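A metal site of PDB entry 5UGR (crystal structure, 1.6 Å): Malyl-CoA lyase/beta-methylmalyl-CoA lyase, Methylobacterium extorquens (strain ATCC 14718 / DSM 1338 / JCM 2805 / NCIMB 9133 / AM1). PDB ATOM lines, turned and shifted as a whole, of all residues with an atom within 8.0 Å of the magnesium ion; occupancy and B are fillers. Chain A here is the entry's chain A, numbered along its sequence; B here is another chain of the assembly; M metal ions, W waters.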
ATOM      1  N   ASP A  42      17.868 -17.963  33.596  1.00  0.00           N
ATOM      2  CA  ASP A  42      17.479 -18.106  32.209  1.00  0.00           C
ATOM      3  C   ASP A  42      17.477 -16.770  31.447  1.00  0.00           C
ATOM      4  O   ASP A  42      16.909 -15.753  31.915  1.00  0.00           O
ATOM      5  CB  ASP A  42      16.077 -18.704  32.189  1.00  0.00           C
ATOM      6  CG  ASP A  42      15.653 -19.229  30.820  1.00  0.00           C
ATOM      7  OD1 ASP A  42      16.530 -19.432  29.933  1.00  0.00           O
ATOM      8  OD2 ASP A  42      14.411 -19.454  30.666  1.00  0.00           O
ATOM      9  N   GLU A  44      16.879 -17.287  27.979  1.00  0.00           N
ATOM     10  CA  GLU A  44      16.332 -17.878  26.748  1.00  0.00           C
ATOM     11  C   GLU A  44      14.805 -18.013  26.830  1.00  0.00           C
ATOM     12  O   GLU A  44      14.100 -17.003  26.933  1.00  0.00           O
ATOM     13  CB  GLU A  44      17.148 -19.173  26.385  1.00  0.00           C
ATOM     14  CG  GLU A  44      16.898 -19.707  24.955  1.00  0.00           C
ATOM     15  CD  GLU A  44      16.285 -21.081  24.834  1.00  0.00           C
ATOM     16  OE1 GLU A  44      15.841 -21.624  25.888  1.00  0.00           O
ATOM     17  OE2 GLU A  44      16.204 -21.580  23.660  1.00  0.00           O
ATOM     18  N   ASP A  45      14.285 -19.249  26.827  1.00  0.00           N
ATOM     19  CA  ASP A  45      12.851 -19.479  26.568  1.00  0.00           C
ATOM     20  C   ASP A  45      11.897 -18.607  27.470  1.00  0.00           C
ATOM     21  O   ASP A  45      10.874 -18.092  27.005  1.00  0.00           O
ATOM     22  CB  ASP A  45      12.471 -20.933  26.820  1.00  0.00           C
ATOM     23  CG  ASP A  45      12.746 -21.889  25.671  1.00  0.00           C
ATOM     24  OD1 ASP A  45      12.728 -21.439  24.490  1.00  0.00           O
ATOM     25  OD2 ASP A  45      12.979 -23.134  25.979  1.00  0.00           O
ATOM     26  N   ALA A  46      12.183 -18.498  28.777  1.00  0.00           N
ATOM     27  CA  ALA A  46      11.268 -17.795  29.671  1.00  0.00           C
ATOM     28  C   ALA A  46      11.326 -16.308  29.609  1.00  0.00           C
ATOM     29  O   ALA A  46      10.561 -15.655  30.309  1.00  0.00           O
ATOM     30  CB  ALA A  46      11.472 -18.270  31.124  1.00  0.00           C
ATOM     31  N   ARG A  76      21.273 -20.231  31.288  1.00  0.00           N
ATOM     32  CA  ARG A  76      20.787 -20.750  29.998  1.00  0.00           C
ATOM     33  C   ARG A  76      20.871 -19.567  29.024  1.00  0.00           C
ATOM     34  O   ARG A  76      20.123 -18.590  29.121  1.00  0.00           O
ATOM     35  CB  ARG A  76      19.430 -21.358  30.005  1.00  0.00           C
ATOM     36  CG  ARG A  76      19.041 -21.876  28.597  1.00  0.00           C
ATOM     37  CD  ARG A  76      17.806 -22.745  28.562  1.00  0.00           C
ATOM     38  NE  ARG A  76      16.577 -22.076  29.034  1.00  0.00           N
ATOM     39  CZ  ARG A  76      15.392 -22.685  29.133  1.00  0.00           C
ATOM     40  NH1 ARG A  76      15.281 -23.954  28.751  1.00  0.00           N
ATOM     41  NH2 ARG A  76      14.333 -22.092  29.694  1.00  0.00           N
ATOM     42  N   PRO A 105      21.314 -24.122  24.782  1.00  0.00           N
ATOM     43  CA  PRO A 105      20.020 -24.616  24.317  1.00  0.00           C
ATOM     44  C   PRO A 105      20.052 -25.132  22.872  1.00  0.00           C
ATOM     45  O   PRO A 105      20.919 -24.736  22.066  1.00  0.00           O
ATOM     46  CB  PRO A 105      19.126 -23.362  24.444  1.00  0.00           C
ATOM     47  CG  PRO A 105      20.070 -22.257  24.043  1.00  0.00           C
ATOM     48  CD  PRO A 105      21.377 -22.641  24.686  1.00  0.00           C
ATOM     49  N   LYS A 106      19.096 -26.037  22.600  1.00  0.00           N
ATOM     50  CA  LYS A 106      18.786 -26.399  21.221  1.00  0.00           C
ATOM     51  C   LYS A 106      19.961 -26.968  20.470  1.00  0.00           C
ATOM     52  O   LYS A 106      20.124 -26.790  19.274  1.00  0.00           O
ATOM     53  CB  LYS A 106      18.151 -25.247  20.443  1.00  0.00           C
ATOM     54  CG  LYS A 106      16.987 -24.597  21.137  1.00  0.00           C
ATOM     55  CD  LYS A 106      16.378 -23.460  20.372  1.00  0.00           C
ATOM     56  CE  LYS A 106      17.367 -22.456  19.760  1.00  0.00           C
ATOM     57  NZ  LYS A 106      16.641 -21.245  19.213  1.00  0.00           N
ATOM     58  N   LEU A 138      21.282 -28.886  26.224  1.00  0.00           N
ATOM     59  CA  LEU A 138      19.885 -29.281  26.069  1.00  0.00           C
ATOM     60  C   LEU A 138      19.682 -30.020  24.758  1.00  0.00           C
ATOM     61  O   LEU A 138      20.031 -29.487  23.668  1.00  0.00           O
ATOM     62  CB  LEU A 138      18.997 -28.041  26.104  1.00  0.00           C
ATOM     63  CG  LEU A 138      18.223 -27.823  27.384  1.00  0.00           C
ATOM     64  CD1 LEU A 138      17.890 -26.373  27.616  1.00  0.00           C
ATOM     65  CD2 LEU A 138      16.996 -28.697  27.434  1.00  0.00           C
ATOM     66  N   ILE A 139      19.179 -31.255  24.876  1.00  0.00           N
ATOM     67  CA  ILE A 139      18.736 -32.051  23.718  1.00  0.00           C
ATOM     68  C   ILE A 139      17.223 -31.864  23.721  1.00  0.00           C
ATOM     69  O   ILE A 139      16.482 -32.465  24.557  1.00  0.00           O
ATOM     70  CB  ILE A 139      19.190 -33.507  23.858  1.00  0.00           C
ATOM     71  CG1 ILE A 139      20.708 -33.604  24.022  1.00  0.00           C
ATOM     72  CG2 ILE A 139      18.691 -34.305  22.651  1.00  0.00           C
ATOM     73  CD1 ILE A 139      21.514 -33.118  22.886  1.00  0.00           C
ATOM     74  N   GLU A 140      16.761 -30.977  22.844  1.00  0.00           N
ATOM     75  CA  GLU A 140      15.372 -30.486  22.887  1.00  0.00           C
ATOM     76  C   GLU A 140      14.826 -30.302  21.465  1.00  0.00           C
ATOM     77  O   GLU A 140      13.842 -29.606  21.285  1.00  0.00           O
ATOM     78  CB  GLU A 140      15.254 -29.193  23.688  1.00  0.00           C
ATOM     79  CG  GLU A 140      16.040 -28.010  23.124  1.00  0.00           C
ATOM     80  CD  GLU A 140      15.840 -26.709  23.899  1.00  0.00           C
ATOM     81  OE1 GLU A 140      14.650 -26.381  24.106  1.00  0.00           O
ATOM     82  OE2 GLU A 140      16.849 -26.076  24.245  1.00  0.00           O
ATOM     83  N   THR A 141      15.496 -30.938  20.497  1.00  0.00           N
ATOM     84  CA  THR A 141      15.053 -30.892  19.124  1.00  0.00           C
ATOM     85  C   THR A 141      15.319 -32.261  18.509  1.00  0.00           C
ATOM     86  O   THR A 141      16.184 -33.033  19.020  1.00  0.00           O
ATOM     87  CB  THR A 141      15.828 -29.840  18.286  1.00  0.00           C
ATOM     88  OG1 THR A 141      17.229 -30.196  18.235  1.00  0.00           O
ATOM     89  CG2 THR A 141      15.669 -28.439  18.815  1.00  0.00           C
ATOM     90  N   GLY A 164      14.996 -31.869  26.988  1.00  0.00           N
ATOM     91  CA  GLY A 164      13.979 -30.808  26.944  1.00  0.00           C
ATOM     92  C   GLY A 164      12.699 -31.307  26.346  1.00  0.00           C
ATOM     93  O   GLY A 164      12.417 -31.085  25.158  1.00  0.00           O
ATOM     94  N   VAL A 165      11.888 -31.967  27.159  1.00  0.00           N
ATOM     95  CA  VAL A 165      10.729 -32.713  26.658  1.00  0.00           C
ATOM     96  C   VAL A 165       9.719 -31.874  25.886  1.00  0.00           C
ATOM     97  O   VAL A 165       9.166 -32.344  24.897  1.00  0.00           O
ATOM     98  CB  VAL A 165      10.078 -33.553  27.793  1.00  0.00           C
ATOM     99  CG1 VAL A 165       9.504 -32.647  28.877  1.00  0.00           C
ATOM    100  CG2 VAL A 165       9.025 -34.502  27.218  1.00  0.00           C
ATOM    101  N   ALA A 166       9.422 -30.660  26.354  1.00  0.00           N
ATOM    102  CA  ALA A 166       8.376 -29.883  25.666  1.00  0.00           C
ATOM    103  C   ALA A 166       8.822 -29.362  24.320  1.00  0.00           C
ATOM    104  O   ALA A 166       8.096 -29.421  23.276  1.00  0.00           O
ATOM    105  CB  ALA A 166       7.896 -28.744  26.557  1.00  0.00           C
ATOM    106  N   ASP A 167      10.059 -28.875  24.278  1.00  0.00           N
ATOM    107  CA  ASP A 167      10.636 -28.424  23.001  1.00  0.00           C
ATOM    108  C   ASP A 167      10.924 -29.588  22.051  1.00  0.00           C
ATOM    109  O   ASP A 167      10.754 -29.452  20.820  1.00  0.00           O
ATOM    110  CB  ASP A 167      11.766 -27.405  23.181  1.00  0.00           C
ATOM    111  CG  ASP A 167      11.227 -26.025  23.574  1.00  0.00           C
ATOM    112  OD1 ASP A 167      10.042 -25.746  23.328  1.00  0.00           O
ATOM    113  OD2 ASP A 167      12.023 -25.190  24.039  1.00  0.00           O
ATOM    114  N   TYR A 168      11.275 -30.739  22.625  1.00  0.00           N
ATOM    115  CA  TYR A 168      11.428 -31.921  21.802  1.00  0.00           C
ATOM    116  C   TYR A 168      10.090 -32.334  21.177  1.00  0.00           C
ATOM    117  O   TYR A 168      10.018 -32.656  19.975  1.00  0.00           O
ATOM    118  CB  TYR A 168      12.017 -33.075  22.603  1.00  0.00           C
ATOM    119  CG  TYR A 168      12.099 -34.377  21.894  1.00  0.00           C
ATOM    120  CD1 TYR A 168      13.147 -34.645  21.046  1.00  0.00           C
ATOM    121  CD2 TYR A 168      11.135 -35.341  22.073  1.00  0.00           C
ATOM    122  CE1 TYR A 168      13.251 -35.862  20.394  1.00  0.00           C
ATOM    123  CE2 TYR A 168      11.213 -36.585  21.405  1.00  0.00           C
ATOM    124  CZ  TYR A 168      12.268 -36.823  20.563  1.00  0.00           C
ATOM    125  OH  TYR A 168      12.400 -38.032  19.920  1.00  0.00           O
ATOM    126  N   PRO A 228      11.605 -30.591  32.108  1.00  0.00           N
ATOM    127  CA  PRO A 228      10.504 -30.051  32.882  1.00  0.00           C
ATOM    128  C   PRO A 228       9.255 -30.920  32.844  1.00  0.00           C
ATOM    129  O   PRO A 228       9.030 -31.643  31.866  1.00  0.00           O
ATOM    130  CB  PRO A 228      10.245 -28.700  32.210  1.00  0.00           C
ATOM    131  CG  PRO A 228      10.670 -28.928  30.772  1.00  0.00           C
ATOM    132  CD  PRO A 228      11.858 -29.843  30.848  1.00  0.00           C
ATOM    133  N   TRP A 254      14.578 -31.513  36.251  1.00  0.00           N
ATOM    134  CA  TRP A 254      14.272 -30.119  36.438  1.00  0.00           C
ATOM    135  C   TRP A 254      13.119 -29.903  37.442  1.00  0.00           C
ATOM    136  O   TRP A 254      12.185 -30.685  37.511  1.00  0.00           O
ATOM    137  CB  TRP A 254      13.879 -29.431  35.129  1.00  0.00           C
ATOM    138  CG  TRP A 254      14.996 -29.284  34.143  1.00  0.00           C
ATOM    139  CD1 TRP A 254      16.166 -30.011  34.041  1.00  0.00           C
ATOM    140  CD2 TRP A 254      14.984 -28.390  33.045  1.00  0.00           C
ATOM    141  NE1 TRP A 254      16.891 -29.586  32.958  1.00  0.00           N
ATOM    142  CE2 TRP A 254      16.187 -28.585  32.319  1.00  0.00           C
ATOM    143  CE3 TRP A 254      14.083 -27.435  32.612  1.00  0.00           C
ATOM    144  CZ2 TRP A 254      16.478 -27.858  31.182  1.00  0.00           C
ATOM    145  CZ3 TRP A 254      14.363 -26.716  31.492  1.00  0.00           C
ATOM    146  CH2 TRP A 254      15.544 -26.923  30.765  1.00  0.00           C
ATOM    147  N   ARG B 301       7.195 -15.098  24.169  1.00  0.00           N
ATOM    148  CA  ARG B 301       8.210 -16.083  23.870  1.00  0.00           C
ATOM    149  C   ARG B 301       8.791 -15.815  22.487  1.00  0.00           C
ATOM    150  O   ARG B 301       8.083 -15.616  21.507  1.00  0.00           O
ATOM    151  CB  ARG B 301       7.639 -17.496  23.888  1.00  0.00           C
ATOM    152  CG  ARG B 301       8.717 -18.525  23.815  1.00  0.00           C
ATOM    153  CD  ARG B 301       8.168 -19.897  24.114  1.00  0.00           C
ATOM    154  NE  ARG B 301       9.268 -20.847  23.964  1.00  0.00           N
ATOM    155  CZ  ARG B 301       9.125 -22.147  23.916  1.00  0.00           C
ATOM    156  NH1 ARG B 301       7.890 -22.696  24.025  1.00  0.00           N
ATOM    157  NH2 ARG B 301      10.187 -22.914  23.724  1.00  0.00           N
ATOM    158  N   ASP B 304      11.671 -19.057  17.176  1.00  0.00           N
ATOM    159  CA  ASP B 304      12.895 -19.163  16.376  1.00  0.00           C
ATOM    160  C   ASP B 304      12.628 -19.637  14.931  1.00  0.00           C
ATOM    161  O   ASP B 304      11.490 -19.992  14.587  1.00  0.00           O
ATOM    162  CB  ASP B 304      13.945 -20.049  17.110  1.00  0.00           C
ATOM    163  CG  ASP B 304      13.539 -21.467  17.303  1.00  0.00           C
ATOM    164  OD1 ASP B 304      12.626 -21.979  16.595  1.00  0.00           O
ATOM    165  OD2 ASP B 304      14.267 -22.173  18.071  1.00  0.00           O
HETATM  166 MG    MG M   1      13.775 -24.788  24.948  1.00  0.00          MG
HETATM  167  O   HOH W   1      14.200 -23.487  23.323  1.00  0.00           O
HETATM  168  O   HOH W   2      15.564 -24.230  25.784  1.00  0.00           O
HETATM  169  O   HOH W   3      13.330 -25.900  26.639  1.00  0.00           O
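The side-chain carboxylate (OE2) of Glu 140 lies within hydrogen-bond range of the backbone NH (N) of Lys 106 (2.8 Å). The backbone carbonyl oxygen (O) of Glu 140 sits at hydrogen-bond distance from the backbone NH (N) of Tyr 168 (3.1 Å). OD1 of Asp 167 lies within salt-bridge range of NH2 of Arg 301 of chain B (2.9 Å). The side-chain carboxylate (OD2) of Asp 45 lies close to the guanidinium group (NH1) of Arg 76, at 3.7 Å. OD1 of Asp 45 is in salt-bridge range of NH2 of Arg 301 of chain B. OE1 of Glu 44 lies within salt-bridge range of NE of Arg 76, at 3.3 Å. The backbone NH (N) of Glu 44 lies within hydrogen-bond range of the side-chain carboxylate (OD1) of Asp 42.
Water W1 bridges OD1 of Asp 45 and OE2 of Glu 44. Water W2 lies within hydrogen-bond range of OE1 of Glu 44 (2.6 Å), OE2 of Glu 140 (2.7 Å) and NH1 of Arg 76 (3.0 Å).
Glu 44 touches the magnesium ion (OE1 to MG, 3.9 Å). Four residues have an atom within 4 Å of the magnesium ion: Glu 44, Asp 45, Glu 140 and Asp 167.
The magnesium ion is bound by the side-chain carboxylate of Glu 140, the side-chain carboxylate of Asp 167, water W2, water W3, the side-chain carboxylate of Asp 45 and water W1. The magnesium ion has six donor atoms within binding distance.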
